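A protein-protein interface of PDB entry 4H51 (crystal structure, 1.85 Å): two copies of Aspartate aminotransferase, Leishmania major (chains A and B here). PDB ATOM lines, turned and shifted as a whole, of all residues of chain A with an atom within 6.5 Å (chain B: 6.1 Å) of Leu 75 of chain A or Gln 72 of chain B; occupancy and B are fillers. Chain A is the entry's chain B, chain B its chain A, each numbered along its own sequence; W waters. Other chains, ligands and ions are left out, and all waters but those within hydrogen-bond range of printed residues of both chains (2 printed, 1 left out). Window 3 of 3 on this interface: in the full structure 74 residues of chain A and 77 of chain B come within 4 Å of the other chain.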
ATOM      1  N   ALA A  70     -35.300  22.822 -22.319  1.00  0.00           N
ATOM      2  CA  ALA A  70     -35.284  23.924 -23.282  1.00  0.00           C
ATOM      3  C   ALA A  70     -34.000  24.765 -23.197  1.00  0.00           C
ATOM      4  O   ALA A  70     -33.522  25.278 -24.239  1.00  0.00           O
ATOM      5  CB  ALA A  70     -36.536  24.802 -23.099  1.00  0.00           C
ATOM      6  N   GLU A  71     -33.425  24.945 -22.003  1.00  0.00           N
ATOM      7  CA  GLU A  71     -32.171  25.693 -21.924  1.00  0.00           C
ATOM      8  C   GLU A  71     -31.079  24.962 -22.738  1.00  0.00           C
ATOM      9  O   GLU A  71     -30.311  25.597 -23.472  1.00  0.00           O
ATOM     10  CB  GLU A  71     -31.693  25.934 -20.476  1.00  0.00           C
ATOM     11  CG  GLU A  71     -32.424  27.028 -19.686  1.00  0.00           C
ATOM     12  CD  GLU A  71     -31.809  28.433 -19.804  1.00  0.00           C
ATOM     13  OE1 GLU A  71     -30.947  28.652 -20.676  1.00  0.00           O
ATOM     14  OE2 GLU A  71     -32.180  29.345 -19.003  1.00  0.00           O
ATOM     15  N   GLN A  72     -31.009  23.654 -22.624  1.00  0.00           N
ATOM     16  CA  GLN A  72     -29.979  22.913 -23.370  1.00  0.00           C
ATOM     17  C   GLN A  72     -30.190  22.954 -24.872  1.00  0.00           C
ATOM     18  O   GLN A  72     -29.230  23.061 -25.657  1.00  0.00           O
ATOM     19  CB  GLN A  72     -29.922  21.455 -22.906  1.00  0.00           C
ATOM     20  CG  GLN A  72     -28.693  20.713 -23.411  1.00  0.00           C
ATOM     21  CD  GLN A  72     -27.354  21.343 -23.017  1.00  0.00           C
ATOM     22  OE1 GLN A  72     -27.026  21.485 -21.838  1.00  0.00           O
ATOM     23  NE2 GLN A  72     -26.553  21.686 -24.026  1.00  0.00           N
ATOM     24  N   LEU A  73     -31.446  22.840 -25.286  1.00  0.00           N
ATOM     25  CA  LEU A  73     -31.755  22.856 -26.708  1.00  0.00           C
ATOM     26  C   LEU A  73     -31.413  24.214 -27.311  1.00  0.00           C
ATOM     27  O   LEU A  73     -30.864  24.284 -28.403  1.00  0.00           O
ATOM     28  CB  LEU A  73     -33.219  22.442 -26.949  1.00  0.00           C
ATOM     29  CG  LEU A  73     -33.449  20.984 -26.480  1.00  0.00           C
ATOM     30  CD1 LEU A  73     -34.934  20.675 -26.604  1.00  0.00           C
ATOM     31  CD2 LEU A  73     -32.543  19.966 -27.222  1.00  0.00           C
ATOM     32  N   LEU A  74     -31.668  25.300 -26.580  1.00  0.00           N
ATOM     33  CA  LEU A  74     -31.283  26.647 -27.053  1.00  0.00           C
ATOM     34  C   LEU A  74     -29.777  26.826 -27.142  1.00  0.00           C
ATOM     35  O   LEU A  74     -29.255  27.434 -28.095  1.00  0.00           O
ATOM     36  CB  LEU A  74     -31.835  27.757 -26.129  1.00  0.00           C
ATOM     37  CG  LEU A  74     -33.245  28.246 -26.326  1.00  0.00           C
ATOM     38  CD1 LEU A  74     -33.497  29.359 -25.295  1.00  0.00           C
ATOM     39  CD2 LEU A  74     -33.386  28.771 -27.750  1.00  0.00           C
ATOM     40  N   LEU A  75     -29.066  26.343 -26.132  1.00  0.00           N
ATOM     41  CA  LEU A  75     -27.624  26.437 -26.141  1.00  0.00           C
ATOM     42  C   LEU A  75     -27.053  25.672 -27.355  1.00  0.00           C
ATOM     43  O   LEU A  75     -26.176  26.180 -28.070  1.00  0.00           O
ATOM     44  CB  LEU A  75     -27.073  25.901 -24.829  1.00  0.00           C
ATOM     45  CG  LEU A  75     -25.657  26.316 -24.483  1.00  0.00           C
ATOM     46  CD1 LEU A  75     -25.486  27.753 -24.844  1.00  0.00           C
ATOM     47  CD2 LEU A  75     -25.355  26.120 -22.996  1.00  0.00           C
ATOM     48  N   ASP A  76     -27.615  24.502 -27.633  1.00  0.00           N
ATOM     49  CA  ASP A  76     -27.158  23.709 -28.751  1.00  0.00           C
ATOM     50  C   ASP A  76     -27.411  24.375 -30.102  1.00  0.00           C
ATOM     51  O   ASP A  76     -26.734  24.046 -31.088  1.00  0.00           O
ATOM     52  CB  ASP A  76     -27.842  22.346 -28.762  1.00  0.00           C
ATOM     53  CG  ASP A  76     -27.435  21.464 -27.603  1.00  0.00           C
ATOM     54  OD1 ASP A  76     -26.428  21.738 -26.930  1.00  0.00           O
ATOM     55  OD2 ASP A  76     -28.208  20.517 -27.344  1.00  0.00           O
ATOM     56  N   MET A  77     -28.383  25.270 -30.162  1.00  0.00           N
ATOM     57  CA  MET A  77     -28.679  26.009 -31.390  1.00  0.00           C
ATOM     58  C   MET A  77     -27.697  27.122 -31.715  1.00  0.00           C
ATOM     59  O   MET A  77     -27.734  27.686 -32.814  1.00  0.00           O
ATOM     60  CB  MET A  77     -30.098  26.556 -31.360  1.00  0.00           C
ATOM     61  CG  MET A  77     -31.199  25.541 -31.587  1.00  0.00           C
ATOM     62  SD  MET A  77     -32.807  26.261 -31.281  1.00  0.00           S
ATOM     63  CE  MET A  77     -33.072  27.211 -32.789  1.00  0.00           C
ATOM     64  N   ASN A  78     -26.812  27.461 -30.774  1.00  0.00           N
ATOM     65  CA  ASN A  78     -25.718  28.415 -31.066  1.00  0.00           C
ATOM     66  C   ASN A  78     -26.282  29.717 -31.688  1.00  0.00           C
ATOM     67  O   ASN A  78     -25.841  30.165 -32.752  1.00  0.00           O
ATOM     68  CB  ASN A  78     -24.658  27.777 -31.966  1.00  0.00           C
ATOM     69  CG  ASN A  78     -23.928  26.597 -31.280  1.00  0.00           C
ATOM     70  OD1 ASN A  78     -23.539  26.712 -30.112  1.00  0.00           O
ATOM     71  ND2 ASN A  78     -23.771  25.439 -31.995  1.00  0.00           N
ATOM     72  N   LEU A  79     -27.247  30.314 -31.002  1.00  0.00           N
ATOM     73  CA  LEU A  79     -27.952  31.496 -31.511  1.00  0.00           C
ATOM     74  C   LEU A  79     -27.181  32.774 -31.316  1.00  0.00           C
ATOM     75  O   LEU A  79     -26.276  32.845 -30.491  1.00  0.00           O
ATOM     76  CB  LEU A  79     -29.291  31.654 -30.808  1.00  0.00           C
ATOM     77  CG  LEU A  79     -30.235  30.475 -30.975  1.00  0.00           C
ATOM     78  CD1 LEU A  79     -31.241  30.462 -29.845  1.00  0.00           C
ATOM     79  CD2 LEU A  79     -30.882  30.514 -32.370  1.00  0.00           C
ATOM     80  N   TYR A  81     -27.319  37.131 -30.598  1.00  0.00           N
ATOM     81  CA  TYR A  81     -27.957  38.041 -29.618  1.00  0.00           C
ATOM     82  C   TYR A  81     -28.369  39.346 -30.289  1.00  0.00           C
ATOM     83  O   TYR A  81     -28.411  40.401 -29.645  1.00  0.00           O
ATOM     84  CB  TYR A  81     -26.948  38.371 -28.502  1.00  0.00           C
ATOM     85  CG  TYR A  81     -26.603  37.183 -27.684  1.00  0.00           C
ATOM     86  CD1 TYR A  81     -27.390  36.805 -26.628  1.00  0.00           C
ATOM     87  CD2 TYR A  81     -25.494  36.417 -27.979  1.00  0.00           C
ATOM     88  CE1 TYR A  81     -27.091  35.691 -25.863  1.00  0.00           C
ATOM     89  CE2 TYR A  81     -25.188  35.295 -27.232  1.00  0.00           C
ATOM     90  CZ  TYR A  81     -25.980  34.961 -26.162  1.00  0.00           C
ATOM     91  OH  TYR A  81     -25.693  33.845 -25.424  1.00  0.00           O
ATOM     92  N   VAL B  67     -19.011  35.368 -24.087  1.00  0.00           N
ATOM     93  CA  VAL B  67     -20.436  35.153 -23.776  1.00  0.00           C
ATOM     94  C   VAL B  67     -20.849  33.691 -23.945  1.00  0.00           C
ATOM     95  O   VAL B  67     -21.587  33.163 -23.124  1.00  0.00           O
ATOM     96  CB  VAL B  67     -21.351  36.053 -24.601  1.00  0.00           C
ATOM     97  CG1 VAL B  67     -22.824  35.630 -24.488  1.00  0.00           C
ATOM     98  CG2 VAL B  67     -21.158  37.514 -24.159  1.00  0.00           C
ATOM     99  N   ARG B  68     -20.382  33.060 -25.015  1.00  0.00           N
ATOM    100  CA  ARG B  68     -20.530  31.593 -25.169  1.00  0.00           C
ATOM    101  C   ARG B  68     -20.030  30.828 -23.967  1.00  0.00           C
ATOM    102  O   ARG B  68     -20.709  29.948 -23.477  1.00  0.00           O
ATOM    103  CB  ARG B  68     -19.800  31.114 -26.417  1.00  0.00           C
ATOM    104  CG  ARG B  68     -20.536  31.480 -27.660  1.00  0.00           C
ATOM    105  CD  ARG B  68     -21.733  30.560 -27.780  1.00  0.00           C
ATOM    106  NE  ARG B  68     -22.397  30.717 -29.065  1.00  0.00           N
ATOM    107  CZ  ARG B  68     -23.602  31.261 -29.269  1.00  0.00           C
ATOM    108  NH1 ARG B  68     -24.354  31.750 -28.285  1.00  0.00           N
ATOM    109  NH2 ARG B  68     -24.049  31.309 -30.512  1.00  0.00           N
ATOM    110  N   LYS B  69     -18.852  31.174 -23.465  1.00  0.00           N
ATOM    111  CA  LYS B  69     -18.348  30.521 -22.273  1.00  0.00           C
ATOM    112  C   LYS B  69     -19.256  30.759 -21.073  1.00  0.00           C
ATOM    113  O   LYS B  69     -19.503  29.832 -20.257  1.00  0.00           O
ATOM    114  CB  LYS B  69     -16.965  31.011 -21.917  1.00  0.00           C
ATOM    115  CG  LYS B  69     -15.834  30.436 -22.739  1.00  0.00           C
ATOM    116  CD  LYS B  69     -14.509  30.963 -22.216  1.00  0.00           C
ATOM    117  CE  LYS B  69     -13.298  30.358 -22.909  1.00  0.00           C
ATOM    118  NZ  LYS B  69     -12.049  30.892 -22.318  1.00  0.00           N
ATOM    119  N   ALA B  70     -19.712  32.002 -20.935  1.00  0.00           N
ATOM    120  CA  ALA B  70     -20.500  32.364 -19.800  1.00  0.00           C
ATOM    121  C   ALA B  70     -21.826  31.574 -19.816  1.00  0.00           C
ATOM    122  O   ALA B  70     -22.283  31.149 -18.755  1.00  0.00           O
ATOM    123  CB  ALA B  70     -20.739  33.875 -19.744  1.00  0.00           C
ATOM    124  N   GLU B  71     -22.427  31.391 -20.997  1.00  0.00           N
ATOM    125  CA  GLU B  71     -23.700  30.668 -21.088  1.00  0.00           C
ATOM    126  C   GLU B  71     -23.566  29.242 -20.500  1.00  0.00           C
ATOM    127  O   GLU B  71     -24.437  28.786 -19.757  1.00  0.00           O
ATOM    128  CB  GLU B  71     -24.223  30.624 -22.541  1.00  0.00           C
ATOM    129  CG  GLU B  71     -24.814  31.923 -23.083  1.00  0.00           C
ATOM    130  CD  GLU B  71     -26.331  32.061 -22.898  1.00  0.00           C
ATOM    131  OE1 GLU B  71     -26.907  31.335 -22.065  1.00  0.00           O
ATOM    132  OE2 GLU B  71     -26.957  32.906 -23.600  1.00  0.00           O
ATOM    133  N   GLN B  72     -22.458  28.560 -20.804  1.00  0.00           N
ATOM    134  CA  GLN B  72     -22.215  27.207 -20.276  1.00  0.00           C
ATOM    135  C   GLN B  72     -21.966  27.198 -18.785  1.00  0.00           C
ATOM    136  O   GLN B  72     -22.493  26.336 -18.078  1.00  0.00           O
ATOM    137  CB  GLN B  72     -21.031  26.517 -20.975  1.00  0.00           C
ATOM    138  CG  GLN B  72     -20.929  25.050 -20.580  1.00  0.00           C
ATOM    139  CD  GLN B  72     -22.089  24.250 -21.117  1.00  0.00           C
ATOM    140  OE1 GLN B  72     -22.314  24.220 -22.317  1.00  0.00           O
ATOM    141  NE2 GLN B  72     -22.818  23.586 -20.240  1.00  0.00           N
ATOM    142  N   LEU B  73     -21.158  28.147 -18.323  1.00  0.00           N
ATOM    143  CA  LEU B  73     -20.880  28.261 -16.916  1.00  0.00           C
ATOM    144  C   LEU B  73     -22.148  28.512 -16.131  1.00  0.00           C
ATOM    145  O   LEU B  73     -22.331  27.949 -15.052  1.00  0.00           O
ATOM    146  CB  LEU B  73     -19.872  29.372 -16.624  1.00  0.00           C
ATOM    147  CG  LEU B  73     -18.476  29.025 -17.177  1.00  0.00           C
ATOM    148  CD1 LEU B  73     -17.675  30.301 -17.294  1.00  0.00           C
ATOM    149  CD2 LEU B  73     -17.746  27.949 -16.363  1.00  0.00           C
ATOM    150  N   LEU B  74     -23.024  29.351 -16.682  1.00  0.00           N
ATOM    151  CA  LEU B  74     -24.302  29.628 -16.000  1.00  0.00           C
ATOM    152  C   LEU B  74     -25.217  28.414 -15.920  1.00  0.00           C
ATOM    153  O   LEU B  74     -25.782  28.107 -14.860  1.00  0.00           O
ATOM    154  CB  LEU B  74     -25.033  30.744 -16.742  1.00  0.00           C
ATOM    155  CG  LEU B  74     -24.613  32.152 -16.471  1.00  0.00           C
ATOM    156  CD1 LEU B  74     -25.637  33.078 -17.176  1.00  0.00           C
ATOM    157  CD2 LEU B  74     -24.572  32.462 -14.972  1.00  0.00           C
ATOM    158  N   LEU B  75     -25.342  27.718 -17.042  1.00  0.00           N
ATOM    159  CA  LEU B  75     -26.168  26.524 -17.124  1.00  0.00           C
ATOM    160  C   LEU B  75     -25.708  25.481 -16.123  1.00  0.00           C
ATOM    161  O   LEU B  75     -26.531  24.853 -15.421  1.00  0.00           O
ATOM    162  CB  LEU B  75     -26.165  25.961 -18.551  1.00  0.00           C
ATOM    163  CG  LEU B  75     -27.530  25.415 -19.009  1.00  0.00           C
ATOM    164  CD1 LEU B  75     -28.571  26.519 -18.746  1.00  0.00           C
ATOM    165  CD2 LEU B  75     -27.546  25.023 -20.489  1.00  0.00           C
ATOM    166  N   ASP B  76     -24.381  25.356 -16.001  1.00  0.00           N
ATOM    167  CA  ASP B  76     -23.794  24.392 -15.069  1.00  0.00           C
ATOM    168  C   ASP B  76     -24.060  24.762 -13.609  1.00  0.00           C
ATOM    169  O   ASP B  76     -23.958  23.915 -12.747  1.00  0.00           O
ATOM    170  CB  ASP B  76     -22.289  24.256 -15.297  1.00  0.00           C
ATOM    171  CG  ASP B  76     -21.956  23.585 -16.641  1.00  0.00           C
ATOM    172  OD1 ASP B  76     -22.813  22.916 -17.222  1.00  0.00           O
ATOM    173  OD2 ASP B  76     -20.830  23.753 -17.109  1.00  0.00           O
ATOM    174  N   MET B  77     -24.386  26.011 -13.319  1.00  0.00           N
ATOM    175  CA  MET B  77     -24.703  26.400 -11.936  1.00  0.00           C
ATOM    176  C   MET B  77     -26.092  25.971 -11.432  1.00  0.00           C
ATOM    177  O   MET B  77     -26.377  26.159 -10.262  1.00  0.00           O
ATOM    178  CB  MET B  77     -24.564  27.902 -11.786  1.00  0.00           C
ATOM    179  CG  MET B  77     -23.146  28.399 -11.905  1.00  0.00           C
ATOM    180  SD  MET B  77     -23.077  30.183 -12.001  1.00  0.00           S
ATOM    181  CE  MET B  77     -21.327  30.408 -12.337  1.00  0.00           C
HETATM  182  O   HOH W   1     -24.673  32.557 -33.678  1.00  0.00           O
HETATM  183  O   HOH W   2     -24.615  21.746 -20.937  1.00  0.00           O
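O of Asn 78 of chain A lies close to NH2 of Arg 68 of chain B, 3.1 Å away. OE2 of Glu 71 of chain B sits at hydrogen-bond distance from OH of Tyr 81 of chain A, 2.4 Å away. NH2 of Arg 68 of chain B is in hydrogen-bond range of O of Leu 79 of chain A, at 2.7 Å.
O of Leu 75 of chain A lies close to OD1 of Asn 78 of chain A, at 3.4 Å. The backbone carbonyl oxygen (O) of Asp 76 of chain A sits at hydrogen-bond distance from the side-chain amide nitrogen (ND2) of Asn 78 of chain A, 3.4 Å away. The side-chain amide nitrogen of Gln 72 of chain B lies within hydrogen-bond range of the side-chain carboxylate of Asp 76 of chain B, 3.1 Å away. The side-chain amide nitrogen (NE2) of Gln 72 of chain A lies within hydrogen-bond range of the side-chain carboxylate (OD1) of Asp 76 of chain A (2.9 Å).
Among the printed residues, pairs that only touch across the chains: Leu 75 of chain A with Leu 75 of chain B, Tyr 81 of chain A with Val 67 of chain B, Glu 71 of chain A with Leu 75 of chain B, Leu 75 of chain A with Gln 72 of chain B, Tyr 81 of chain A with Arg 68 of chain B, Gln 72 of chain A with Leu 75 of chain B and Leu 75 of chain A with Glu 71 of chain B.
Printed residues of chain B within 4 Å of Gln 72 of chain A: Leu 75 (3.8 Å). Of the printed residues of chain B, Asn 78 of chain A touches Arg 68 (3.0 Å). Of the printed residues of chain A, Arg 68 of chain B touches Asn 78 (3.0 Å), Leu 79 (2.7 Å) and Tyr 81 (3.8 Å). Of chain A, only Leu 75 (3.6 Å) comes within 4 Å of Gln 72 of chain B. Printed residues of chain A within 4 Å of Leu 75 of chain B: Glu 71 (3.6 Å), Gln 72 (3.8 Å) and Leu 75 (3.5 Å). The nearest printed residue of chain B that does not touch Leu 75 of chain A is Arg 68 of chain B (5.4 Å).
Hydrophobic or aromatic side chains of chain A that line the printed part of chain B: Leu 75 and Tyr 81. Among the printed residues, no Asp or Glu carboxylate lies within 4 Å of a Lys or Arg side-chain nitrogen of the other chain.
Glu 71 of chain A touches Leu 75 of chain B, and with the chains exchanged Leu 75 of chain A touches Glu 71 of chain B. Gln 72 of chain A touches Leu 75 of chain B, and with the chains exchanged Leu 75 of chain A touches Gln 72 of chain B. Leu 75 of chain A touches its own counterpart, Leu 75 of chain B. Of the 10 pairs that touch across the chains among the printed residues, 5 have their exchanged pair printed and touching as well.
Water W2 lies within hydrogen-bond range of OE1 of Gln 72 of chain A (2.6 Å) and NE2 of Gln 72 of chain B (2.7 Å). Water W1 lies within hydrogen-bond range of the backbone carbonyl oxygen (O) of Asn 78 of chain A (2.8 Å) and the guanidinium group (NH2) of Arg 68 of chain B (3.5 Å).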
